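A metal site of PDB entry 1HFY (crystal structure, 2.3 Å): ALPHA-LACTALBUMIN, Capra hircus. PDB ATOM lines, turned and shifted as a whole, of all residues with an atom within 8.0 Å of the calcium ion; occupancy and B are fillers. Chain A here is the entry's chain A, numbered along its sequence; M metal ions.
OG1 of Thr 86 is in hydrogen-bond range of OD1 of Asp 84 (2.5 Å).
Five residues have an atom within 4 Å of the calcium ion: Lys 79, Asp 82, Asp 84, Asp 87 and Asp 88.
The nearest printed residue that does not touch the calcium ion is Phe 80 (4.1 Å).
The calcium ion is bound by O of Asp 84 (2.3 Å), O of Lys 79 (2.3 Å), OD1 of Asp 87 (2.4 Å), OD1 of Asp 88 (2.5 Å) and OD1 of Asp 82 (2.5 Å).
The calcium ion has five donor atoms within binding distance.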
ATOM      1  N   THR A  38      15.187  11.502   3.216  1.00  0.00           N
ATOM      2  CA  THR A  38      15.814  10.211   3.482  1.00  0.00           C
ATOM      3  C   THR A  38      14.838   9.074   3.714  1.00  0.00           C
ATOM      4  O   THR A  38      15.177   7.919   3.530  1.00  0.00           O
ATOM      5  CB  THR A  38      16.725  10.292   4.707  1.00  0.00           C
ATOM      6  OG1 THR A  38      15.939  10.670   5.850  1.00  0.00           O
ATOM      7  CG2 THR A  38      17.810  11.356   4.474  1.00  0.00           C
ATOM      8  N   ILE A  75      20.839  -6.086   0.002  1.00  0.00           N
ATOM      9  CA  ILE A  75      20.432  -5.440   1.239  1.00  0.00           C
ATOM     10  C   ILE A  75      18.924  -5.367   1.359  1.00  0.00           C
ATOM     11  O   ILE A  75      18.222  -5.494   0.360  1.00  0.00           O
ATOM     12  CB  ILE A  75      20.960  -3.996   1.228  1.00  0.00           C
ATOM     13  CG1 ILE A  75      20.920  -3.402   2.626  1.00  0.00           C
ATOM     14  CG2 ILE A  75      20.157  -3.184   0.230  1.00  0.00           C
ATOM     15  CD1 ILE A  75      21.619  -2.054   2.735  1.00  0.00           C
ATOM     16  N   SER A  76      18.406  -5.172   2.571  1.00  0.00           N
ATOM     17  CA  SER A  76      16.964  -5.041   2.715  1.00  0.00           C
ATOM     18  C   SER A  76      16.649  -3.574   2.469  1.00  0.00           C
ATOM     19  O   SER A  76      17.300  -2.679   3.002  1.00  0.00           O
ATOM     20  CB  SER A  76      16.481  -5.455   4.104  1.00  0.00           C
ATOM     21  OG  SER A  76      17.059  -4.599   5.060  1.00  0.00           O
ATOM     22  N   CYS A  77      15.587  -3.338   1.715  1.00  0.00           N
ATOM     23  CA  CYS A  77      15.190  -2.003   1.345  1.00  0.00           C
ATOM     24  C   CYS A  77      15.064  -0.971   2.457  1.00  0.00           C
ATOM     25  O   CYS A  77      15.350   0.190   2.236  1.00  0.00           O
ATOM     26  CB  CYS A  77      13.914  -2.066   0.525  1.00  0.00           C
ATOM     27  SG  CYS A  77      14.105  -3.063  -0.974  1.00  0.00           S
ATOM     28  N   ASP A  78      14.714  -1.409   3.649  1.00  0.00           N
ATOM     29  CA  ASP A  78      14.537  -0.483   4.764  1.00  0.00           C
ATOM     30  C   ASP A  78      15.806   0.103   5.343  1.00  0.00           C
ATOM     31  O   ASP A  78      15.777   0.964   6.222  1.00  0.00           O
ATOM     32  CB  ASP A  78      13.612  -1.062   5.859  1.00  0.00           C
ATOM     33  CG  ASP A  78      14.117  -2.339   6.455  1.00  0.00           C
ATOM     34  OD1 ASP A  78      14.426  -3.291   5.695  1.00  0.00           O
ATOM     35  OD2 ASP A  78      14.190  -2.405   7.697  1.00  0.00           O
ATOM     36  N   LYS A  79      16.948  -0.349   4.825  1.00  0.00           N
ATOM     37  CA  LYS A  79      18.225   0.212   5.251  1.00  0.00           C
ATOM     38  C   LYS A  79      18.382   1.574   4.560  1.00  0.00           C
ATOM     39  O   LYS A  79      19.259   2.366   4.887  1.00  0.00           O
ATOM     40  CB  LYS A  79      19.352  -0.715   4.849  1.00  0.00           C
ATOM     41  CG  LYS A  79      19.559  -1.828   5.818  1.00  0.00           C
ATOM     42  CD  LYS A  79      19.928  -1.264   7.180  1.00  0.00           C
ATOM     43  CE  LYS A  79      20.730  -2.287   7.971  1.00  0.00           C
ATOM     44  NZ  LYS A  79      20.067  -3.629   7.953  1.00  0.00           N
ATOM     45  N   PHE A  80      17.521   1.817   3.579  1.00  0.00           N
ATOM     46  CA  PHE A  80      17.517   3.074   2.848  1.00  0.00           C
ATOM     47  C   PHE A  80      16.511   4.073   3.437  1.00  0.00           C
ATOM     48  O   PHE A  80      16.250   5.106   2.830  1.00  0.00           O
ATOM     49  CB  PHE A  80      17.192   2.817   1.381  1.00  0.00           C
ATOM     50  CG  PHE A  80      18.126   1.857   0.718  1.00  0.00           C
ATOM     51  CD1 PHE A  80      19.463   1.811   1.080  1.00  0.00           C
ATOM     52  CD2 PHE A  80      17.670   1.018  -0.277  1.00  0.00           C
ATOM     53  CE1 PHE A  80      20.336   0.938   0.463  1.00  0.00           C
ATOM     54  CE2 PHE A  80      18.536   0.130  -0.908  1.00  0.00           C
ATOM     55  CZ  PHE A  80      19.874   0.088  -0.538  1.00  0.00           C
ATOM     56  N   LEU A  81      15.992   3.805   4.619  1.00  0.00           N
ATOM     57  CA  LEU A  81      15.033   4.724   5.214  1.00  0.00           C
ATOM     58  C   LEU A  81      15.504   5.359   6.484  1.00  0.00           C
ATOM     59  O   LEU A  81      14.736   5.996   7.186  1.00  0.00           O
ATOM     60  CB  LEU A  81      13.695   4.044   5.447  1.00  0.00           C
ATOM     61  CG  LEU A  81      13.014   3.608   4.170  1.00  0.00           C
ATOM     62  CD1 LEU A  81      11.807   2.779   4.516  1.00  0.00           C
ATOM     63  CD2 LEU A  81      12.659   4.796   3.316  1.00  0.00           C
ATOM     64  N   ASP A  82      16.768   5.144   6.823  1.00  0.00           N
ATOM     65  CA  ASP A  82      17.315   5.770   8.014  1.00  0.00           C
ATOM     66  C   ASP A  82      18.159   6.994   7.673  1.00  0.00           C
ATOM     67  O   ASP A  82      18.279   7.365   6.507  1.00  0.00           O
ATOM     68  CB  ASP A  82      18.055   4.749   8.918  1.00  0.00           C
ATOM     69  CG  ASP A  82      19.167   3.999   8.209  1.00  0.00           C
ATOM     70  OD1 ASP A  82      19.839   4.578   7.310  1.00  0.00           O
ATOM     71  OD2 ASP A  82      19.391   2.825   8.573  1.00  0.00           O
ATOM     72  N   ASP A  83      18.812   7.553   8.676  1.00  0.00           N
ATOM     73  CA  ASP A  83      19.633   8.741   8.502  1.00  0.00           C
ATOM     74  C   ASP A  83      21.055   8.503   8.068  1.00  0.00           C
ATOM     75  O   ASP A  83      21.753   9.456   7.708  1.00  0.00           O
ATOM     76  CB  ASP A  83      19.621   9.571   9.782  1.00  0.00           C
ATOM     77  CG  ASP A  83      18.234  10.046  10.140  1.00  0.00           C
ATOM     78  OD1 ASP A  83      17.474  10.412   9.208  1.00  0.00           O
ATOM     79  OD2 ASP A  83      17.883  10.026  11.348  1.00  0.00           O
ATOM     80  N   ASP A  84      21.498   7.247   8.120  1.00  0.00           N
ATOM     81  CA  ASP A  84      22.850   6.896   7.705  1.00  0.00           C
ATOM     82  C   ASP A  84      22.895   6.617   6.191  1.00  0.00           C
ATOM     83  O   ASP A  84      22.356   5.606   5.705  1.00  0.00           O
ATOM     84  CB  ASP A  84      23.355   5.690   8.510  1.00  0.00           C
ATOM     85  CG  ASP A  84      24.836   5.465   8.357  1.00  0.00           C
ATOM     86  OD1 ASP A  84      25.487   6.198   7.592  1.00  0.00           O
ATOM     87  OD2 ASP A  84      25.359   4.550   9.011  1.00  0.00           O
ATOM     88  N   LEU A  85      23.510   7.531   5.433  1.00  0.00           N
ATOM     89  CA  LEU A  85      23.565   7.405   3.986  1.00  0.00           C
ATOM     90  C   LEU A  85      24.639   6.489   3.423  1.00  0.00           C
ATOM     91  O   LEU A  85      24.591   6.118   2.246  1.00  0.00           O
ATOM     92  CB  LEU A  85      23.585   8.780   3.324  1.00  0.00           C
ATOM     93  CG  LEU A  85      22.363   9.685   3.570  1.00  0.00           C
ATOM     94  CD1 LEU A  85      22.393  10.864   2.608  1.00  0.00           C
ATOM     95  CD2 LEU A  85      21.040   8.907   3.387  1.00  0.00           C
ATOM     96  N   THR A  86      25.524   6.018   4.277  1.00  0.00           N
ATOM     97  CA  THR A  86      26.604   5.129   3.864  1.00  0.00           C
ATOM     98  C   THR A  86      26.135   4.019   2.903  1.00  0.00           C
ATOM     99  O   THR A  86      26.578   3.936   1.772  1.00  0.00           O
ATOM    100  CB  THR A  86      27.259   4.480   5.092  1.00  0.00           C
ATOM    101  OG1 THR A  86      27.426   5.468   6.108  1.00  0.00           O
ATOM    102  CG2 THR A  86      28.638   3.915   4.749  1.00  0.00           C
ATOM    103  N   ASP A  87      25.218   3.173   3.348  1.00  0.00           N
ATOM    104  CA  ASP A  87      24.766   2.095   2.481  1.00  0.00           C
ATOM    105  C   ASP A  87      23.974   2.552   1.256  1.00  0.00           C
ATOM    106  O   ASP A  87      23.978   1.871   0.232  1.00  0.00           O
ATOM    107  CB  ASP A  87      24.015   1.026   3.292  1.00  0.00           C
ATOM    108  CG  ASP A  87      22.972   1.590   4.221  1.00  0.00           C
ATOM    109  OD1 ASP A  87      22.587   2.774   4.041  1.00  0.00           O
ATOM    110  OD2 ASP A  87      22.537   0.862   5.137  1.00  0.00           O
ATOM    111  N   ASP A  88      23.362   3.736   1.335  1.00  0.00           N
ATOM    112  CA  ASP A  88      22.558   4.281   0.228  1.00  0.00           C
ATOM    113  C   ASP A  88      23.497   4.635  -0.919  1.00  0.00           C
ATOM    114  O   ASP A  88      23.201   4.397  -2.106  1.00  0.00           O
ATOM    115  CB  ASP A  88      21.845   5.578   0.659  1.00  0.00           C
ATOM    116  CG  ASP A  88      20.704   5.350   1.623  1.00  0.00           C
ATOM    117  OD1 ASP A  88      20.952   5.009   2.796  1.00  0.00           O
ATOM    118  OD2 ASP A  88      19.549   5.572   1.206  1.00  0.00           O
ATOM    119  N   ILE A  89      24.627   5.234  -0.539  1.00  0.00           N
ATOM    120  CA  ILE A  89      25.675   5.671  -1.459  1.00  0.00           C
ATOM    121  C   ILE A  89      26.371   4.516  -2.162  1.00  0.00           C
ATOM    122  O   ILE A  89      26.708   4.598  -3.339  1.00  0.00           O
ATOM    123  CB  ILE A  89      26.670   6.555  -0.682  1.00  0.00           C
ATOM    124  CG1 ILE A  89      25.958   7.878  -0.305  1.00  0.00           C
ATOM    125  CG2 ILE A  89      27.988   6.696  -1.443  1.00  0.00           C
ATOM    126  CD1 ILE A  89      26.747   8.858   0.582  1.00  0.00           C
HETATM  127 CA    CA M   1      20.825   4.048   5.064  1.00  0.00          CA
